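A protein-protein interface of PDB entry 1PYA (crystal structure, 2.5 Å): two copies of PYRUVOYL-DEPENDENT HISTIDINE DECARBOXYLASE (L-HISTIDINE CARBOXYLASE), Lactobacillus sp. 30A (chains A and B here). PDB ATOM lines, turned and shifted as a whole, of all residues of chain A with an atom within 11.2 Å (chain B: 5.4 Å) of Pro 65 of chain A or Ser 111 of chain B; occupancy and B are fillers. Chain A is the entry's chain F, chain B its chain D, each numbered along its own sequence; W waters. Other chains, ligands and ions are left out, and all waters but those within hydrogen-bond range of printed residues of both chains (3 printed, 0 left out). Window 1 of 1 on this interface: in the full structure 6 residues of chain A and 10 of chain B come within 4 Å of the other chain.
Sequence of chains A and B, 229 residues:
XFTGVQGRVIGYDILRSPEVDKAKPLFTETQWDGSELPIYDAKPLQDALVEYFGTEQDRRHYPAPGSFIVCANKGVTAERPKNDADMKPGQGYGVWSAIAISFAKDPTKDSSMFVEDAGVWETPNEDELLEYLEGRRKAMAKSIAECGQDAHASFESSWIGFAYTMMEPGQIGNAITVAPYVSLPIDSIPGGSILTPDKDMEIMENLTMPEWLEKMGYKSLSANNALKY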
ATOM      1  N   PHE A  53     -10.192 -17.958   1.613  1.00  0.00           N
ATOM      2  CA  PHE A  53     -10.842 -17.819   2.919  1.00  0.00           C
ATOM      3  C   PHE A  53     -12.315 -18.125   2.849  1.00  0.00           C
ATOM      4  O   PHE A  53     -12.881 -18.625   3.819  1.00  0.00           O
ATOM      5  CB  PHE A  53     -10.698 -16.393   3.501  1.00  0.00           C
ATOM      6  CG  PHE A  53      -9.360 -16.067   4.148  1.00  0.00           C
ATOM      7  CD1 PHE A  53      -8.348 -17.006   4.209  1.00  0.00           C
ATOM      8  CD2 PHE A  53      -9.175 -14.802   4.670  1.00  0.00           C
ATOM      9  CE1 PHE A  53      -7.159 -16.649   4.796  1.00  0.00           C
ATOM     10  CE2 PHE A  53      -7.980 -14.458   5.253  1.00  0.00           C
ATOM     11  CZ  PHE A  53      -6.971 -15.382   5.316  1.00  0.00           C
ATOM     12  N   GLU A  56     -18.629 -15.222   4.393  1.00  0.00           N
ATOM     13  CA  GLU A  56     -19.323 -15.600   5.629  1.00  0.00           C
ATOM     14  C   GLU A  56     -20.350 -16.657   5.310  1.00  0.00           C
ATOM     15  O   GLU A  56     -20.622 -17.528   6.130  1.00  0.00           O
ATOM     16  CB  GLU A  56     -19.972 -14.363   6.218  1.00  0.00           C
ATOM     17  CG  GLU A  56     -20.518 -14.429   7.659  1.00  0.00           C
ATOM     18  CD  GLU A  56     -21.879 -15.088   7.759  1.00  0.00           C
ATOM     19  OE1 GLU A  56     -22.753 -14.803   6.936  1.00  0.00           O
ATOM     20  OE2 GLU A  56     -22.048 -15.928   8.642  1.00  0.00           O
ATOM     21  N   ARG A  59     -17.908 -20.526   3.860  1.00  0.00           N
ATOM     22  CA  ARG A  59     -16.659 -20.359   4.563  1.00  0.00           C
ATOM     23  C   ARG A  59     -15.695 -21.423   4.090  1.00  0.00           C
ATOM     24  O   ARG A  59     -16.097 -22.555   3.944  1.00  0.00           O
ATOM     25  CB  ARG A  59     -16.879 -20.483   6.081  1.00  0.00           C
ATOM     26  CG  ARG A  59     -18.123 -19.788   6.573  1.00  0.00           C
ATOM     27  CD  ARG A  59     -17.967 -18.614   7.481  1.00  0.00           C
ATOM     28  NE  ARG A  59     -18.131 -18.984   8.869  1.00  0.00           N
ATOM     29  CZ  ARG A  59     -18.848 -18.253   9.741  1.00  0.00           C
ATOM     30  NH1 ARG A  59     -19.660 -17.266   9.363  1.00  0.00           N
ATOM     31  NH2 ARG A  59     -18.809 -18.570  11.033  1.00  0.00           N
ATOM     32  N   ARG A  60     -14.426 -21.115   3.840  1.00  0.00           N
ATOM     33  CA  ARG A  60     -13.469 -22.088   3.356  1.00  0.00           C
ATOM     34  C   ARG A  60     -12.303 -22.087   4.358  1.00  0.00           C
ATOM     35  O   ARG A  60     -12.492 -22.442   5.510  1.00  0.00           O
ATOM     36  CB  ARG A  60     -13.031 -21.648   1.940  1.00  0.00           C
ATOM     37  CG  ARG A  60     -13.583 -22.413   0.774  1.00  0.00           C
ATOM     38  CD  ARG A  60     -14.696 -21.841  -0.063  1.00  0.00           C
ATOM     39  NE  ARG A  60     -14.120 -21.327  -1.281  1.00  0.00           N
ATOM     40  CZ  ARG A  60     -14.703 -21.334  -2.489  1.00  0.00           C
ATOM     41  NH1 ARG A  60     -15.863 -21.923  -2.754  1.00  0.00           N
ATOM     42  NH2 ARG A  60     -14.032 -20.752  -3.480  1.00  0.00           N
ATOM     43  N   HIS A  61     -11.060 -21.666   4.066  1.00  0.00           N
ATOM     44  CA  HIS A  61      -9.958 -21.850   5.006  1.00  0.00           C
ATOM     45  C   HIS A  61      -9.674 -20.556   5.737  1.00  0.00           C
ATOM     46  O   HIS A  61      -8.564 -20.015   5.766  1.00  0.00           O
ATOM     47  CB  HIS A  61      -8.755 -22.359   4.208  1.00  0.00           C
ATOM     48  CG  HIS A  61      -9.141 -23.697   3.589  1.00  0.00           C
ATOM     49  ND1 HIS A  61      -9.395 -24.833   4.240  1.00  0.00           N
ATOM     50  CD2 HIS A  61      -9.416 -23.937   2.255  1.00  0.00           C
ATOM     51  CE1 HIS A  61      -9.806 -25.736   3.383  1.00  0.00           C
ATOM     52  NE2 HIS A  61      -9.825 -25.183   2.188  1.00  0.00           N
ATOM     53  N   TYR A  62     -10.731 -20.043   6.352  1.00  0.00           N
ATOM     54  CA  TYR A  62     -10.642 -18.755   7.064  1.00  0.00           C
ATOM     55  C   TYR A  62      -9.919 -18.917   8.394  1.00  0.00           C
ATOM     56  O   TYR A  62      -9.703 -20.058   8.850  1.00  0.00           O
ATOM     57  CB  TYR A  62     -12.094 -18.162   7.285  1.00  0.00           C
ATOM     58  CG  TYR A  62     -12.988 -19.002   8.189  1.00  0.00           C
ATOM     59  CD1 TYR A  62     -13.619 -20.091   7.676  1.00  0.00           C
ATOM     60  CD2 TYR A  62     -13.139 -18.677   9.515  1.00  0.00           C
ATOM     61  CE1 TYR A  62     -14.392 -20.874   8.490  1.00  0.00           C
ATOM     62  CE2 TYR A  62     -13.917 -19.457  10.343  1.00  0.00           C
ATOM     63  CZ  TYR A  62     -14.528 -20.554   9.812  1.00  0.00           C
ATOM     64  OH  TYR A  62     -15.281 -21.361  10.609  1.00  0.00           O
ATOM     65  N   PRO A  63      -9.496 -17.827   9.036  1.00  0.00           N
ATOM     66  CA  PRO A  63      -8.743 -17.893  10.284  1.00  0.00           C
ATOM     67  C   PRO A  63      -9.560 -18.527  11.418  1.00  0.00           C
ATOM     68  O   PRO A  63     -10.779 -18.348  11.484  1.00  0.00           O
ATOM     69  CB  PRO A  63      -8.336 -16.423  10.495  1.00  0.00           C
ATOM     70  CG  PRO A  63      -8.318 -15.758   9.133  1.00  0.00           C
ATOM     71  CD  PRO A  63      -9.536 -16.451   8.515  1.00  0.00           C
ATOM     72  N   ALA A  64      -8.952 -19.314  12.297  1.00  0.00           N
ATOM     73  CA  ALA A  64      -9.682 -19.970  13.374  1.00  0.00           C
ATOM     74  C   ALA A  64     -10.385 -18.951  14.291  1.00  0.00           C
ATOM     75  O   ALA A  64      -9.852 -17.867  14.543  1.00  0.00           O
ATOM     76  CB  ALA A  64      -8.695 -20.808  14.223  1.00  0.00           C
ATOM     77  N   PRO A  65     -11.532 -19.266  14.899  1.00  0.00           N
ATOM     78  CA  PRO A  65     -12.202 -18.339  15.794  1.00  0.00           C
ATOM     79  C   PRO A  65     -11.397 -18.124  17.063  1.00  0.00           C
ATOM     80  O   PRO A  65     -10.990 -19.058  17.776  1.00  0.00           O
ATOM     81  CB  PRO A  65     -13.575 -18.946  15.997  1.00  0.00           C
ATOM     82  CG  PRO A  65     -13.513 -20.354  15.514  1.00  0.00           C
ATOM     83  CD  PRO A  65     -12.418 -20.342  14.484  1.00  0.00           C
ATOM     84  N   GLY A  66     -11.070 -16.850  17.227  1.00  0.00           N
ATOM     85  CA  GLY A  66     -10.333 -16.370  18.369  1.00  0.00           C
ATOM     86  C   GLY A  66      -8.832 -16.400  18.114  1.00  0.00           C
ATOM     87  O   GLY A  66      -8.070 -16.194  19.062  1.00  0.00           O
ATOM     88  N   SER A  67      -8.352 -16.609  16.886  1.00  0.00           N
ATOM     89  CA  SER A  67      -6.913 -16.692  16.652  1.00  0.00           C
ATOM     90  C   SER A  67      -6.316 -15.303  16.637  1.00  0.00           C
ATOM     91  O   SER A  67      -7.029 -14.311  16.390  1.00  0.00           O
ATOM     92  CB  SER A  67      -6.622 -17.376  15.312  1.00  0.00           C
ATOM     93  OG  SER A  67      -7.186 -16.739  14.165  1.00  0.00           O
ATOM     94  N   PHE A  68      -5.022 -15.197  16.877  1.00  0.00           N
ATOM     95  CA  PHE A  68      -4.347 -13.930  16.795  1.00  0.00           C
ATOM     96  C   PHE A  68      -3.738 -13.791  15.433  1.00  0.00           C
ATOM     97  O   PHE A  68      -2.815 -14.534  15.136  1.00  0.00           O
ATOM     98  CB  PHE A  68      -3.299 -13.868  17.888  1.00  0.00           C
ATOM     99  CG  PHE A  68      -3.978 -13.492  19.196  1.00  0.00           C
ATOM    100  CD1 PHE A  68      -4.749 -14.429  19.878  1.00  0.00           C
ATOM    101  CD2 PHE A  68      -3.847 -12.198  19.666  1.00  0.00           C
ATOM    102  CE1 PHE A  68      -5.392 -14.063  21.036  1.00  0.00           C
ATOM    103  CE2 PHE A  68      -4.509 -11.865  20.834  1.00  0.00           C
ATOM    104  CZ  PHE A  68      -5.280 -12.778  21.523  1.00  0.00           C
ATOM    105  N   ILE A  69      -4.239 -12.944  14.543  1.00  0.00           N
ATOM    106  CA  ILE A  69      -3.686 -12.788  13.212  1.00  0.00           C
ATOM    107  C   ILE A  69      -3.103 -11.373  13.110  1.00  0.00           C
ATOM    108  O   ILE A  69      -3.831 -10.374  13.131  1.00  0.00           O
ATOM    109  CB  ILE A  69      -4.786 -12.941  12.102  1.00  0.00           C
ATOM    110  CG1 ILE A  69      -5.661 -14.185  12.268  1.00  0.00           C
ATOM    111  CG2 ILE A  69      -4.071 -13.029  10.766  1.00  0.00           C
ATOM    112  CD1 ILE A  69      -4.998 -15.586  12.321  1.00  0.00           C
ATOM    113  N   PHE B   2     -11.619 -11.285  21.013  1.00  0.00           N
ATOM    114  CA  PHE B   2     -12.254 -12.593  20.959  1.00  0.00           C
ATOM    115  C   PHE B   2     -11.467 -13.607  21.785  1.00  0.00           C
ATOM    116  O   PHE B   2     -10.229 -13.515  21.893  1.00  0.00           O
ATOM    117  CB  PHE B   2     -12.331 -13.104  19.508  1.00  0.00           C
ATOM    118  CG  PHE B   2     -13.233 -12.272  18.600  1.00  0.00           C
ATOM    119  CD1 PHE B   2     -14.599 -12.501  18.607  1.00  0.00           C
ATOM    120  CD2 PHE B   2     -12.711 -11.244  17.809  1.00  0.00           C
ATOM    121  CE1 PHE B   2     -15.411 -11.686  17.843  1.00  0.00           C
ATOM    122  CE2 PHE B   2     -13.545 -10.432  17.056  1.00  0.00           C
ATOM    123  CZ  PHE B   2     -14.900 -10.647  17.083  1.00  0.00           C
ATOM    124  N   THR B   3     -12.171 -14.576  22.366  1.00  0.00           N
ATOM    125  CA  THR B   3     -11.552 -15.712  23.057  1.00  0.00           C
ATOM    126  C   THR B   3     -12.250 -16.849  22.304  1.00  0.00           C
ATOM    127  O   THR B   3     -13.503 -16.933  22.337  1.00  0.00           O
ATOM    128  CB  THR B   3     -11.965 -15.975  24.522  1.00  0.00           C
ATOM    129  OG1 THR B   3     -12.357 -14.759  25.150  1.00  0.00           O
ATOM    130  CG2 THR B   3     -10.840 -16.734  25.205  1.00  0.00           C
ATOM    131  N   GLY B   4     -11.526 -17.713  21.611  1.00  0.00           N
ATOM    132  CA  GLY B   4     -12.198 -18.727  20.834  1.00  0.00           C
ATOM    133  C   GLY B   4     -11.827 -20.109  21.293  1.00  0.00           C
ATOM    134  O   GLY B   4     -11.613 -20.353  22.491  1.00  0.00           O
ATOM    135  N   VAL B   5     -11.608 -20.962  20.274  1.00  0.00           N
ATOM    136  CA  VAL B   5     -11.415 -22.412  20.472  1.00  0.00           C
ATOM    137  C   VAL B   5     -10.180 -22.733  21.312  1.00  0.00           C
ATOM    138  O   VAL B   5     -10.041 -23.828  21.858  1.00  0.00           O
ATOM    139  CB  VAL B   5     -11.358 -23.149  19.059  1.00  0.00           C
ATOM    140  CG1 VAL B   5     -12.672 -22.883  18.294  1.00  0.00           C
ATOM    141  CG2 VAL B   5     -10.218 -22.651  18.175  1.00  0.00           C
ATOM    142  N   GLN B   6      -9.249 -21.809  21.473  1.00  0.00           N
ATOM    143  CA  GLN B   6      -8.058 -21.993  22.297  1.00  0.00           C
ATOM    144  C   GLN B   6      -8.187 -21.517  23.741  1.00  0.00           C
ATOM    145  O   GLN B   6      -7.256 -21.749  24.539  1.00  0.00           O
ATOM    146  CB  GLN B   6      -6.886 -21.224  21.708  1.00  0.00           C
ATOM    147  CG  GLN B   6      -6.428 -21.745  20.366  1.00  0.00           C
ATOM    148  CD  GLN B   6      -5.588 -20.730  19.654  1.00  0.00           C
ATOM    149  OE1 GLN B   6      -6.146 -19.967  18.872  1.00  0.00           O
ATOM    150  NE2 GLN B   6      -4.281 -20.665  19.823  1.00  0.00           N
ATOM    151  N   SER B 102     -19.060 -12.109  26.066  1.00  0.00           N
ATOM    152  CA  SER B 102     -20.249 -12.908  25.918  1.00  0.00           C
ATOM    153  C   SER B 102     -19.855 -14.253  25.310  1.00  0.00           C
ATOM    154  O   SER B 102     -19.118 -14.303  24.324  1.00  0.00           O
ATOM    155  CB  SER B 102     -21.247 -12.125  25.090  1.00  0.00           C
ATOM    156  OG  SER B 102     -20.864 -11.732  23.808  1.00  0.00           O
ATOM    157  N   ALA B 104     -19.917 -18.030  23.746  1.00  0.00           N
ATOM    158  CA  ALA B 104     -20.570 -18.690  22.610  1.00  0.00           C
ATOM    159  C   ALA B 104     -21.340 -19.907  23.065  1.00  0.00           C
ATOM    160  O   ALA B 104     -20.861 -20.622  23.965  1.00  0.00           O
ATOM    161  CB  ALA B 104     -19.585 -19.210  21.564  1.00  0.00           C
ATOM    162  N   THR B 108     -17.207 -24.755  19.568  1.00  0.00           N
ATOM    163  CA  THR B 108     -16.326 -25.402  18.606  1.00  0.00           C
ATOM    164  C   THR B 108     -16.476 -24.705  17.268  1.00  0.00           C
ATOM    165  O   THR B 108     -15.587 -24.845  16.436  1.00  0.00           O
ATOM    166  CB  THR B 108     -16.673 -26.882  18.440  1.00  0.00           C
ATOM    167  OG1 THR B 108     -18.053 -26.908  18.065  1.00  0.00           O
ATOM    168  CG2 THR B 108     -16.488 -27.728  19.713  1.00  0.00           C
ATOM    169  N   LYS B 109     -17.596 -24.003  17.002  1.00  0.00           N
ATOM    170  CA  LYS B 109     -17.806 -23.312  15.738  1.00  0.00           C
ATOM    171  C   LYS B 109     -17.592 -21.834  15.941  1.00  0.00           C
ATOM    172  O   LYS B 109     -16.912 -21.230  15.114  1.00  0.00           O
ATOM    173  CB  LYS B 109     -19.202 -23.352  15.149  1.00  0.00           C
ATOM    174  CG  LYS B 109     -19.992 -24.627  15.106  1.00  0.00           C
ATOM    175  CD  LYS B 109     -19.436 -25.720  14.218  1.00  0.00           C
ATOM    176  CE  LYS B 109     -20.105 -27.065  14.541  1.00  0.00           C
ATOM    177  NZ  LYS B 109     -19.800 -27.505  15.896  1.00  0.00           N
ATOM    178  N   ASP B 110     -18.158 -21.215  16.986  1.00  0.00           N
ATOM    179  CA  ASP B 110     -18.051 -19.764  17.128  1.00  0.00           C
ATOM    180  C   ASP B 110     -17.154 -19.309  18.239  1.00  0.00           C
ATOM    181  O   ASP B 110     -16.974 -20.016  19.233  1.00  0.00           O
ATOM    182  CB  ASP B 110     -19.376 -19.127  17.400  1.00  0.00           C
ATOM    183  CG  ASP B 110     -20.468 -19.473  16.411  1.00  0.00           C
ATOM    184  OD1 ASP B 110     -20.264 -19.340  15.212  1.00  0.00           O
ATOM    185  OD2 ASP B 110     -21.545 -19.850  16.845  1.00  0.00           O
ATOM    186  N   SER B 111     -16.581 -18.141  18.102  1.00  0.00           N
ATOM    187  CA  SER B 111     -15.778 -17.562  19.188  1.00  0.00           C
ATOM    188  C   SER B 111     -16.672 -16.812  20.190  1.00  0.00           C
ATOM    189  O   SER B 111     -17.793 -16.381  19.871  1.00  0.00           O
ATOM    190  CB  SER B 111     -14.767 -16.598  18.593  1.00  0.00           C
ATOM    191  OG  SER B 111     -13.785 -16.163  19.516  1.00  0.00           O
ATOM    192  N   SER B 112     -16.174 -16.714  21.419  1.00  0.00           N
ATOM    193  CA  SER B 112     -16.799 -15.885  22.415  1.00  0.00           C
ATOM    194  C   SER B 112     -16.255 -14.515  22.112  1.00  0.00           C
ATOM    195  O   SER B 112     -15.158 -14.389  21.550  1.00  0.00           O
ATOM    196  CB  SER B 112     -16.398 -16.374  23.791  1.00  0.00           C
ATOM    197  OG  SER B 112     -17.184 -17.541  24.072  1.00  0.00           O
ATOM    198  N   MET B 113     -16.963 -13.461  22.472  1.00  0.00           N
ATOM    199  CA  MET B 113     -16.581 -12.129  22.044  1.00  0.00           C
ATOM    200  C   MET B 113     -16.438 -11.138  23.165  1.00  0.00           C
ATOM    201  O   MET B 113     -17.183 -11.191  24.157  1.00  0.00           O
ATOM    202  CB  MET B 113     -17.627 -11.655  21.050  1.00  0.00           C
ATOM    203  CG  MET B 113     -17.419 -10.292  20.426  1.00  0.00           C
ATOM    204  SD  MET B 113     -18.910  -9.832  19.531  1.00  0.00           S
ATOM    205  CE  MET B 113     -18.621 -10.844  18.126  1.00  0.00           C
ATOM    206  N   ALA B 153     -23.302 -15.933  14.941  1.00  0.00           N
ATOM    207  CA  ALA B 153     -22.855 -16.558  16.166  1.00  0.00           C
ATOM    208  C   ALA B 153     -23.878 -16.287  17.275  1.00  0.00           C
ATOM    209  O   ALA B 153     -24.338 -15.138  17.445  1.00  0.00           O
ATOM    210  CB  ALA B 153     -21.528 -15.962  16.559  1.00  0.00           C
ATOM    211  N   PHE B 155     -24.778 -16.290  21.318  1.00  0.00           N
ATOM    212  CA  PHE B 155     -24.155 -16.292  22.619  1.00  0.00           C
ATOM    213  C   PHE B 155     -25.183 -16.783  23.634  1.00  0.00           C
ATOM    214  O   PHE B 155     -26.396 -16.680  23.455  1.00  0.00           O
ATOM    215  CB  PHE B 155     -23.659 -14.870  22.926  1.00  0.00           C
ATOM    216  CG  PHE B 155     -22.626 -14.424  21.909  1.00  0.00           C
ATOM    217  CD1 PHE B 155     -21.403 -15.084  21.813  1.00  0.00           C
ATOM    218  CD2 PHE B 155     -22.907 -13.370  21.061  1.00  0.00           C
ATOM    219  CE1 PHE B 155     -20.474 -14.696  20.865  1.00  0.00           C
ATOM    220  CE2 PHE B 155     -21.962 -12.992  20.115  1.00  0.00           C
ATOM    221  CZ  PHE B 155     -20.756 -13.651  20.008  1.00  0.00           C
HETATM  222  O   HOH W   1     -18.937 -17.710  13.623  1.00  0.00           O
HETATM  223  O   HOH W   2      -8.958 -19.765  19.554  1.00  0.00           O
HETATM  224  O   HOH W   3     -16.684 -19.776  12.575  1.00  0.00           O
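O of Pro 65 of chain A touches CA of Gly 4 of chain B (3.3 Å).
O of Lys 109 of chain B touches CG of Pro 65 of chain A, at 3.5 Å.
Pro 65 of chain A touches Ser 111 of chain B (CB to CB, 3.7 Å).
Gly 66 of chain A touches Phe 2 of chain B.
Gly 4 of chain B touches Gly 66 of chain A.
N of Gly 66 of chain A touches OG of Ser 111 of chain B, 3.6 Å away.
O of Thr 3 of chain B is in hydrogen-bond range of OG of Ser 111 of chain B (2.9 Å).
OG1 of Thr 108 of chain B lies within hydrogen-bond range of NZ of Lys 109 of chain B (2.8 Å).
The backbone NH (N) of Gly 4 of chain B lies close to the side-chain hydroxyl (OG) of Ser 111 of chain B, 3.4 Å away.
Of chain B, only Gly 4, Val 5, Lys 109 and Ser 111 come within 4 Å of Pro 65 of chain A.
Of chain A, only Pro 65 and Gly 66 come within 4 Å of Ser 111 of chain B.
Of chain A, only Pro 65 comes within 4 Å of Val 5 of chain B.
No residue of chain A comes within 4 Å of Ser 112 of chain B.
No residue of chain A comes within 4 Å of Met 113 of chain B.
Printed residues of chain A within 4 Å of Lys 109 of chain B: Pro 65 (3.5 Å).
Of the printed residues of chain B, Gly 66 of chain A touches Phe 2 (3.99 Å), Gly 4 (3.7 Å) and Ser 111 (3.6 Å).
Printed residues of chain A within 4 Å of Phe 2 of chain B: Gly 66 (3.99 Å).
Ser 67 of chain A touches none of the printed residues of chain B.
The nearest residue of chain B that does not touch Pro 65 of chain A is Asp 110 of chain B (4.2 Å).
N of Val 5 of chain B is in hydrogen-bond range of O of Pro 65 of chain A, 3.2 Å away.
Hydrophobic or aromatic side chains of chain A within 4 Å of the printed part of chain B: Pro 65.
Hydrophobic or aromatic side chains of chain B within 4 Å of the printed part of chain A: Phe 2 and Val 5.
Among the printed residues, 7 pairs touch across the chains.
Among the printed residues, no Asp or Glu carboxylate lies within 4 Å of a Lys or Arg side-chain nitrogen of the other chain.
No position is printed for both chains.
Of the 7 pairs that touch across the chains among the printed residues, none has its exchanged pair printed and touching as well.
Water W1 lies within hydrogen-bond range of OD1 of Asp 110 of chain B and NH2 of Arg 59 of chain A.
Water W2 lies within hydrogen-bond range of the backbone carbonyl oxygen (O) of Pro 65 of chain A (2.8 Å), the backbone NH (N) of Gln 6 of chain B (2.8 Å) and the backbone NH (N) of Val 5 of chain B (3.0 Å).
Water W3 lies within hydrogen-bond range of NH2 of Arg 59 of chain A, OH of Tyr 62 of chain A and O of Lys 109 of chain B.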
